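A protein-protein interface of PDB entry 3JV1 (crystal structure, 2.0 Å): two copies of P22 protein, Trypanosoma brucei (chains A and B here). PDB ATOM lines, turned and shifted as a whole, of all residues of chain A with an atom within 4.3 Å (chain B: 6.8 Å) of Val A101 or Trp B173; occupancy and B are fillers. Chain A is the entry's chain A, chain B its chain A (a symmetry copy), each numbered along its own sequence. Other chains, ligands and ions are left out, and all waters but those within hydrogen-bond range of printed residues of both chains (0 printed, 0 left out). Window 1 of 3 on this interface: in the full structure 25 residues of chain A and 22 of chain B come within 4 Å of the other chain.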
ATOM      1  N   LEU A  85     -24.743  -0.912 -22.059  1.00  0.00           N
ATOM      2  CA  LEU A  85     -24.846  -2.071 -21.190  1.00  0.00           C
ATOM      3  C   LEU A  85     -26.237  -2.552 -21.597  1.00  0.00           C
ATOM      4  O   LEU A  85     -27.209  -1.802 -21.475  1.00  0.00           O
ATOM      5  CB  LEU A  85     -24.862  -1.647 -19.720  1.00  0.00           C
ATOM      6  CG  LEU A  85     -23.954  -2.373 -18.725  1.00  0.00           C
ATOM      7  CD1 LEU A  85     -24.247  -1.858 -17.322  1.00  0.00           C
ATOM      8  CD2 LEU A  85     -24.158  -3.870 -18.803  1.00  0.00           C
ATOM      9  N   VAL A  86     -26.332  -3.781 -22.094  1.00  0.00           N
ATOM     10  CA  VAL A  86     -27.605  -4.320 -22.544  1.00  0.00           C
ATOM     11  C   VAL A  86     -28.093  -5.504 -21.714  1.00  0.00           C
ATOM     12  O   VAL A  86     -27.465  -6.558 -21.691  1.00  0.00           O
ATOM     13  CB  VAL A  86     -27.511  -4.740 -24.030  1.00  0.00           C
ATOM     14  CG1 VAL A  86     -28.882  -5.156 -24.547  1.00  0.00           C
ATOM     15  CG2 VAL A  86     -26.964  -3.578 -24.860  1.00  0.00           C
ATOM     16  N   PHE A  87     -29.222  -5.314 -21.039  1.00  0.00           N
ATOM     17  CA  PHE A  87     -29.824  -6.341 -20.196  1.00  0.00           C
ATOM     18  C   PHE A  87     -30.937  -7.086 -20.928  1.00  0.00           C
ATOM     19  O   PHE A  87     -31.928  -6.477 -21.351  1.00  0.00           O
ATOM     20  CB  PHE A  87     -30.416  -5.707 -18.935  1.00  0.00           C
ATOM     21  CG  PHE A  87     -29.393  -5.080 -18.023  1.00  0.00           C
ATOM     22  CD1 PHE A  87     -28.833  -5.811 -16.975  1.00  0.00           C
ATOM     23  CD2 PHE A  87     -28.987  -3.765 -18.218  1.00  0.00           C
ATOM     24  CE1 PHE A  87     -27.885  -5.233 -16.136  1.00  0.00           C
ATOM     25  CE2 PHE A  87     -28.036  -3.173 -17.382  1.00  0.00           C
ATOM     26  CZ  PHE A  87     -27.484  -3.910 -16.337  1.00  0.00           C
ATOM     27  N   ILE A  98     -33.494 -10.853 -14.823  1.00  0.00           N
ATOM     28  CA  ILE A  98     -32.369 -10.664 -15.718  1.00  0.00           C
ATOM     29  C   ILE A  98     -31.974 -12.025 -16.289  1.00  0.00           C
ATOM     30  O   ILE A  98     -31.684 -12.955 -15.540  1.00  0.00           O
ATOM     31  CB  ILE A  98     -31.156 -10.068 -14.979  1.00  0.00           C
ATOM     32  CG1 ILE A  98     -31.548  -8.758 -14.299  1.00  0.00           C
ATOM     33  CG2 ILE A  98     -30.026  -9.827 -15.961  1.00  0.00           C
ATOM     34  CD1 ILE A  98     -30.533  -8.288 -13.283  1.00  0.00           C
ATOM     35  N   ASN A 100     -29.823 -12.140 -19.299  1.00  0.00           N
ATOM     36  CA  ASN A 100     -28.504 -11.917 -19.879  1.00  0.00           C
ATOM     37  C   ASN A 100     -28.040 -10.491 -19.624  1.00  0.00           C
ATOM     38  O   ASN A 100     -28.847  -9.590 -19.440  1.00  0.00           O
ATOM     39  CB  ASN A 100     -28.532 -12.143 -21.401  1.00  0.00           C
ATOM     40  CG  ASN A 100     -28.767 -13.594 -21.784  1.00  0.00           C
ATOM     41  OD1 ASN A 100     -27.872 -14.430 -21.675  1.00  0.00           O
ATOM     42  ND2 ASN A 100     -29.977 -13.896 -22.235  1.00  0.00           N
ATOM     43  N   VAL A 101     -26.726 -10.309 -19.607  1.00  0.00           N
ATOM     44  CA  VAL A 101     -26.110  -9.001 -19.433  1.00  0.00           C
ATOM     45  C   VAL A 101     -24.971  -8.958 -20.439  1.00  0.00           C
ATOM     46  O   VAL A 101     -24.004  -9.715 -20.325  1.00  0.00           O
ATOM     47  CB  VAL A 101     -25.513  -8.795 -18.029  1.00  0.00           C
ATOM     48  CG1 VAL A 101     -24.811  -7.433 -17.971  1.00  0.00           C
ATOM     49  CG2 VAL A 101     -26.600  -8.867 -16.981  1.00  0.00           C
ATOM     50  N   CYS A 102     -25.107  -8.094 -21.439  1.00  0.00           N
ATOM     51  CA  CYS A 102     -24.098  -7.946 -22.475  1.00  0.00           C
ATOM     52  C   CYS A 102     -23.544  -6.538 -22.440  1.00  0.00           C
ATOM     53  O   CYS A 102     -24.191  -5.609 -21.943  1.00  0.00           O
ATOM     54  CB  CYS A 102     -24.706  -8.159 -23.865  1.00  0.00           C
ATOM     55  SG  CYS A 102     -25.698  -9.629 -24.029  1.00  0.00           S
ATOM     56  N   PHE A 103     -22.335  -6.387 -22.964  1.00  0.00           N
ATOM     57  CA  PHE A 103     -21.737  -5.075 -23.060  1.00  0.00           C
ATOM     58  C   PHE A 103     -21.434  -4.828 -24.530  1.00  0.00           C
ATOM     59  O   PHE A 103     -20.871  -5.683 -25.205  1.00  0.00           O
ATOM     60  CB  PHE A 103     -20.447  -4.954 -22.265  1.00  0.00           C
ATOM     61  CG  PHE A 103     -19.930  -3.546 -22.215  1.00  0.00           C
ATOM     62  CD1 PHE A 103     -20.542  -2.604 -21.399  1.00  0.00           C
ATOM     63  CD2 PHE A 103     -18.886  -3.140 -23.041  1.00  0.00           C
ATOM     64  CE1 PHE A 103     -20.125  -1.273 -21.406  1.00  0.00           C
ATOM     65  CE2 PHE A 103     -18.464  -1.811 -23.054  1.00  0.00           C
ATOM     66  CZ  PHE A 103     -19.088  -0.879 -22.233  1.00  0.00           C
ATOM     67  N   TYR A 125     -20.304 -11.708 -27.945  1.00  0.00           N
ATOM     68  CA  TYR A 125     -20.322 -12.357 -26.641  1.00  0.00           C
ATOM     69  C   TYR A 125     -21.626 -11.965 -25.965  1.00  0.00           C
ATOM     70  O   TYR A 125     -21.995 -10.789 -25.951  1.00  0.00           O
ATOM     71  CB  TYR A 125     -19.135 -11.880 -25.801  1.00  0.00           C
ATOM     72  CG  TYR A 125     -19.041 -12.509 -24.428  1.00  0.00           C
ATOM     73  CD1 TYR A 125     -19.066 -13.895 -24.268  1.00  0.00           C
ATOM     74  CD2 TYR A 125     -18.882 -11.717 -23.292  1.00  0.00           C
ATOM     75  CE1 TYR A 125     -18.935 -14.478 -23.007  1.00  0.00           C
ATOM     76  CE2 TYR A 125     -18.744 -12.288 -22.031  1.00  0.00           C
ATOM     77  CZ  TYR A 125     -18.772 -13.665 -21.898  1.00  0.00           C
ATOM     78  OH  TYR A 125     -18.633 -14.222 -20.652  1.00  0.00           O
ATOM     79  N   MET A 126     -22.323 -12.950 -25.412  1.00  0.00           N
ATOM     80  CA  MET A 126     -23.603 -12.703 -24.762  1.00  0.00           C
ATOM     81  C   MET A 126     -23.508 -12.633 -23.242  1.00  0.00           C
ATOM     82  O   MET A 126     -24.519 -12.726 -22.545  1.00  0.00           O
ATOM     83  CB  MET A 126     -24.589 -13.790 -25.169  1.00  0.00           C
ATOM     84  CG  MET A 126     -24.881 -13.820 -26.664  1.00  0.00           C
ATOM     85  SD  MET A 126     -25.654 -12.286 -27.221  1.00  0.00           S
ATOM     86  CE  MET A 126     -27.256 -12.441 -26.452  1.00  0.00           C
ATOM     87  N   GLY A 127     -22.293 -12.460 -22.738  1.00  0.00           N
ATOM     88  CA  GLY A 127     -22.090 -12.394 -21.303  1.00  0.00           C
ATOM     89  C   GLY A 127     -22.159 -13.773 -20.680  1.00  0.00           C
ATOM     90  O   GLY A 127     -22.470 -14.745 -21.369  1.00  0.00           O
ATOM     91  N   PRO A 128     -21.880 -13.895 -19.376  1.00  0.00           N
ATOM     92  CA  PRO A 128     -21.923 -15.188 -18.691  1.00  0.00           C
ATOM     93  C   PRO A 128     -23.342 -15.626 -18.345  1.00  0.00           C
ATOM     94  O   PRO A 128     -24.285 -14.827 -18.375  1.00  0.00           O
ATOM     95  CB  PRO A 128     -21.111 -14.925 -17.431  1.00  0.00           C
ATOM     96  CG  PRO A 128     -21.537 -13.527 -17.081  1.00  0.00           C
ATOM     97  CD  PRO A 128     -21.469 -12.827 -18.441  1.00  0.00           C
ATOM     98  N   PHE A 141     -26.046  -5.659 -10.009  1.00  0.00           N
ATOM     99  CA  PHE A 141     -26.687  -5.375 -11.293  1.00  0.00           C
ATOM    100  C   PHE A 141     -28.136  -4.959 -11.067  1.00  0.00           C
ATOM    101  O   PHE A 141     -28.598  -3.975 -11.649  1.00  0.00           O
ATOM    102  CB  PHE A 141     -26.659  -6.601 -12.213  1.00  0.00           C
ATOM    103  CG  PHE A 141     -25.405  -6.725 -13.033  1.00  0.00           C
ATOM    104  CD1 PHE A 141     -24.966  -5.665 -13.819  1.00  0.00           C
ATOM    105  CD2 PHE A 141     -24.679  -7.909 -13.046  1.00  0.00           C
ATOM    106  CE1 PHE A 141     -23.818  -5.778 -14.615  1.00  0.00           C
ATOM    107  CE2 PHE A 141     -23.528  -8.038 -13.837  1.00  0.00           C
ATOM    108  CZ  PHE A 141     -23.099  -6.965 -14.624  1.00  0.00           C
ATOM    109  N   THR B  11     -17.628  -5.713  -9.904  1.00  0.00           N
ATOM    110  CA  THR B  11     -16.983  -6.194 -11.122  1.00  0.00           C
ATOM    111  C   THR B  11     -15.467  -6.315 -10.934  1.00  0.00           C
ATOM    112  O   THR B  11     -14.846  -7.257 -11.422  1.00  0.00           O
ATOM    113  CB  THR B  11     -17.302  -5.277 -12.342  1.00  0.00           C
ATOM    114  OG1 THR B  11     -17.097  -3.906 -11.986  1.00  0.00           O
ATOM    115  CG2 THR B  11     -18.761  -5.460 -12.780  1.00  0.00           C
ATOM    116  N   GLU B  14     -14.770  -9.450  -8.917  1.00  0.00           N
ATOM    117  CA  GLU B  14     -14.908 -10.656  -9.717  1.00  0.00           C
ATOM    118  C   GLU B  14     -13.713 -10.820 -10.640  1.00  0.00           C
ATOM    119  O   GLU B  14     -13.177 -11.915 -10.766  1.00  0.00           O
ATOM    120  CB  GLU B  14     -16.216 -10.615 -10.510  1.00  0.00           C
ATOM    121  CG  GLU B  14     -16.457 -11.803 -11.442  1.00  0.00           C
ATOM    122  CD  GLU B  14     -16.368 -13.162 -10.756  1.00  0.00           C
ATOM    123  OE1 GLU B  14     -16.327 -13.218  -9.505  1.00  0.00           O
ATOM    124  OE2 GLU B  14     -16.345 -14.179 -11.483  1.00  0.00           O
ATOM    125  N   ALA B 168     -11.524 -15.276 -22.104  1.00  0.00           N
ATOM    126  CA  ALA B 168     -10.978 -13.956 -22.383  1.00  0.00           C
ATOM    127  C   ALA B 168     -12.117 -12.939 -22.521  1.00  0.00           C
ATOM    128  O   ALA B 168     -12.023 -11.820 -22.029  1.00  0.00           O
ATOM    129  CB  ALA B 168     -10.151 -13.995 -23.663  1.00  0.00           C
ATOM    130  N   ASP B 169     -13.194 -13.334 -23.196  1.00  0.00           N
ATOM    131  CA  ASP B 169     -14.332 -12.442 -23.380  1.00  0.00           C
ATOM    132  C   ASP B 169     -14.977 -12.112 -22.043  1.00  0.00           C
ATOM    133  O   ASP B 169     -15.436 -10.992 -21.827  1.00  0.00           O
ATOM    134  CB  ASP B 169     -15.385 -13.068 -24.307  1.00  0.00           C
ATOM    135  CG  ASP B 169     -14.962 -13.059 -25.766  1.00  0.00           C
ATOM    136  OD1 ASP B 169     -14.002 -12.340 -26.119  1.00  0.00           O
ATOM    137  OD2 ASP B 169     -15.609 -13.765 -26.563  1.00  0.00           O
ATOM    138  N   TYR B 170     -15.003 -13.093 -21.152  1.00  0.00           N
ATOM    139  CA  TYR B 170     -15.587 -12.907 -19.830  1.00  0.00           C
ATOM    140  C   TYR B 170     -14.822 -11.870 -19.027  1.00  0.00           C
ATOM    141  O   TYR B 170     -15.424 -11.023 -18.379  1.00  0.00           O
ATOM    142  CB  TYR B 170     -15.602 -14.220 -19.047  1.00  0.00           C
ATOM    143  CG  TYR B 170     -16.121 -14.041 -17.641  1.00  0.00           C
ATOM    144  CD1 TYR B 170     -17.380 -13.486 -17.414  1.00  0.00           C
ATOM    145  CD2 TYR B 170     -15.356 -14.418 -16.535  1.00  0.00           C
ATOM    146  CE1 TYR B 170     -17.870 -13.311 -16.128  1.00  0.00           C
ATOM    147  CE2 TYR B 170     -15.839 -14.246 -15.235  1.00  0.00           C
ATOM    148  CZ  TYR B 170     -17.097 -13.692 -15.043  1.00  0.00           C
ATOM    149  OH  TYR B 170     -17.590 -13.510 -13.775  1.00  0.00           O
ATOM    150  N   GLU B 171     -13.497 -11.940 -19.062  1.00  0.00           N
ATOM    151  CA  GLU B 171     -12.679 -10.986 -18.324  1.00  0.00           C
ATOM    152  C   GLU B 171     -12.763  -9.596 -18.942  1.00  0.00           C
ATOM    153  O   GLU B 171     -12.723  -8.596 -18.236  1.00  0.00           O
ATOM    154  CB  GLU B 171     -11.219 -11.439 -18.291  1.00  0.00           C
ATOM    155  CG  GLU B 171     -11.024 -12.796 -17.652  1.00  0.00           C
ATOM    156  CD  GLU B 171      -9.563 -13.178 -17.526  1.00  0.00           C
ATOM    157  OE1 GLU B 171      -9.279 -14.387 -17.375  1.00  0.00           O
ATOM    158  OE2 GLU B 171      -8.705 -12.269 -17.563  1.00  0.00           O
ATOM    159  N   GLU B 172     -12.867  -9.538 -20.263  1.00  0.00           N
ATOM    160  CA  GLU B 172     -12.962  -8.260 -20.950  1.00  0.00           C
ATOM    161  C   GLU B 172     -14.341  -7.667 -20.632  1.00  0.00           C
ATOM    162  O   GLU B 172     -14.500  -6.451 -20.514  1.00  0.00           O
ATOM    163  CB  GLU B 172     -12.777  -8.481 -22.452  1.00  0.00           C
ATOM    164  CG  GLU B 172     -12.496  -7.228 -23.258  1.00  0.00           C
ATOM    165  CD  GLU B 172     -13.755  -6.532 -23.699  1.00  0.00           C
ATOM    166  OE1 GLU B 172     -14.734  -7.247 -24.007  1.00  0.00           O
ATOM    167  OE2 GLU B 172     -13.762  -5.280 -23.753  1.00  0.00           O
ATOM    168  N   TRP B 173     -15.323  -8.552 -20.474  1.00  0.00           N
ATOM    169  CA  TRP B 173     -16.694  -8.176 -20.131  1.00  0.00           C
ATOM    170  C   TRP B 173     -16.681  -7.477 -18.765  1.00  0.00           C
ATOM    171  O   TRP B 173     -17.187  -6.371 -18.619  1.00  0.00           O
ATOM    172  CB  TRP B 173     -17.552  -9.443 -20.082  1.00  0.00           C
ATOM    173  CG  TRP B 173     -18.995  -9.259 -19.690  1.00  0.00           C
ATOM    174  CD1 TRP B 173     -20.026  -8.893 -20.501  1.00  0.00           C
ATOM    175  CD2 TRP B 173     -19.569  -9.531 -18.406  1.00  0.00           C
ATOM    176  NE1 TRP B 173     -21.211  -8.933 -19.809  1.00  0.00           N
ATOM    177  CE2 TRP B 173     -20.958  -9.321 -18.518  1.00  0.00           C
ATOM    178  CE3 TRP B 173     -19.041  -9.934 -17.170  1.00  0.00           C
ATOM    179  CZ2 TRP B 173     -21.835  -9.502 -17.440  1.00  0.00           C
ATOM    180  CZ3 TRP B 173     -19.911 -10.114 -16.097  1.00  0.00           C
ATOM    181  CH2 TRP B 173     -21.295  -9.898 -16.241  1.00  0.00           C
ATOM    182  N   LEU B 174     -16.075  -8.120 -17.774  1.00  0.00           N
ATOM    183  CA  LEU B 174     -15.980  -7.554 -16.423  1.00  0.00           C
ATOM    184  C   LEU B 174     -15.297  -6.189 -16.430  1.00  0.00           C
ATOM    185  O   LEU B 174     -15.787  -5.231 -15.834  1.00  0.00           O
ATOM    186  CB  LEU B 174     -15.191  -8.491 -15.506  1.00  0.00           C
ATOM    187  CG  LEU B 174     -15.812  -9.844 -15.156  1.00  0.00           C
ATOM    188  CD1 LEU B 174     -14.783 -10.735 -14.468  1.00  0.00           C
ATOM    189  CD2 LEU B 174     -17.018  -9.619 -14.258  1.00  0.00           C
ATOM    190  N   SER B 175     -14.158  -6.118 -17.112  1.00  0.00           N
ATOM    191  CA  SER B 175     -13.377  -4.892 -17.204  1.00  0.00           C
ATOM    192  C   SER B 175     -14.103  -3.746 -17.897  1.00  0.00           C
ATOM    193  O   SER B 175     -14.062  -2.606 -17.431  1.00  0.00           O
ATOM    194  CB  SER B 175     -12.073  -5.161 -17.944  1.00  0.00           C
ATOM    195  OG  SER B 175     -11.338  -3.960 -18.102  1.00  0.00           O
ATOM    196  N   SER B 176     -14.756  -4.034 -19.014  1.00  0.00           N
ATOM    197  CA  SER B 176     -15.460  -2.976 -19.726  1.00  0.00           C
ATOM    198  C   SER B 176     -16.674  -2.471 -18.944  1.00  0.00           C
ATOM    199  O   SER B 176     -16.991  -1.280 -18.994  1.00  0.00           O
ATOM    200  CB  SER B 176     -15.856  -3.438 -21.143  1.00  0.00           C
ATOM    201  OG  SER B 176     -16.577  -4.653 -21.125  1.00  0.00           O
ATOM    202  N   ILE B 177     -17.351  -3.354 -18.210  1.00  0.00           N
ATOM    203  CA  ILE B 177     -18.503  -2.911 -17.431  1.00  0.00           C
ATOM    204  C   ILE B 177     -18.015  -2.062 -16.264  1.00  0.00           C
ATOM    205  O   ILE B 177     -18.641  -1.073 -15.903  1.00  0.00           O
ATOM    206  CB  ILE B 177     -19.350  -4.098 -16.902  1.00  0.00           C
ATOM    207  CG1 ILE B 177     -20.039  -4.805 -18.071  1.00  0.00           C
ATOM    208  CG2 ILE B 177     -20.419  -3.593 -15.932  1.00  0.00           C
ATOM    209  CD1 ILE B 177     -20.752  -6.077 -17.682  1.00  0.00           C
ATOM    210  N   ASN B 178     -16.882  -2.457 -15.689  1.00  0.00           N
ATOM    211  CA  ASN B 178     -16.276  -1.723 -14.583  1.00  0.00           C
ATOM    212  C   ASN B 178     -15.939  -0.295 -15.030  1.00  0.00           C
ATOM    213  O   ASN B 178     -16.268   0.675 -14.351  1.00  0.00           O
ATOM    214  CB  ASN B 178     -14.999  -2.429 -14.133  1.00  0.00           C
ATOM    215  CG  ASN B 178     -14.271  -1.671 -13.046  1.00  0.00           C
ATOM    216  OD1 ASN B 178     -14.640  -1.735 -11.868  1.00  0.00           O
ATOM    217  ND2 ASN B 178     -13.239  -0.933 -13.435  1.00  0.00           N
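The backbone carbonyl oxygen of Val A101 is in hydrogen-bond range of the indole nitrogen of Trp B173, at 2.9 Å.
The side-chain carboxylate (OE2) of Glu B14 sits at hydrogen-bond distance from the side-chain hydroxyl (OH) of Tyr B170 (2.7 Å).
O of Glu B172 sits at hydrogen-bond distance from OG of Ser B176.
O of Trp B173 is in hydrogen-bond range of OG of Ser B176 (3.1 Å).
Among the printed residues, pairs that only touch across the chains: Phe A103 with Ser B176, Tyr A125 with Tyr B170, Pro A128 with Trp B173, Tyr A125 with Asp B169, Tyr A125 with Trp B173, Phe A141 with Trp B173, Pro A128 with Tyr B170, Gly A127 with Trp B173 and Phe A141 with Ile B177.
Of the printed residues of chain B, Tyr A125 touches Asp B169, Tyr B170 and Trp B173.
Printed residues of chain B within 4 Å of Phe A141: Trp B173 (3.8 Å) and Ile B177 (3.96 Å).
Of chain A, only Val A101, Tyr A125, Gly A127, Pro A128 and Phe A141 come within 4 Å of Trp B173.
Printed residues of chain A within 4 Å of Ser B176: Phe A103.
Of the printed residues of chain A, Ile B177 touches Phe A141 (3.96 Å).
The nearest residue of chain B that does not touch Val A101 is Ile B177 (4.3 Å).
Of the 13 printed residues of chain B, 5 touch a printed residue of chain A.
Printed residues of chain B that touch a printed residue of chain A: Asp B169, Tyr B170, Trp B173, Ser B176 and Ile B177.
Hydrophobic or aromatic side chains of chain B that line the printed part of chain A: Tyr B170, Trp B173 and Ile B177.
Of the 13 printed residues of chain A, 6 touch a printed residue of chain B.
Along chain A the printed residues that touch a printed residue of chain B span positions 101 to 141.
Among the printed residues, no Asp or Glu carboxylate lies within 4 Å of a Lys or Arg side-chain nitrogen of the other chain.
No position is printed for both chains.
Of the 10 pairs that touch across the chains among the printed residues, none has its exchanged pair printed and touching as well.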
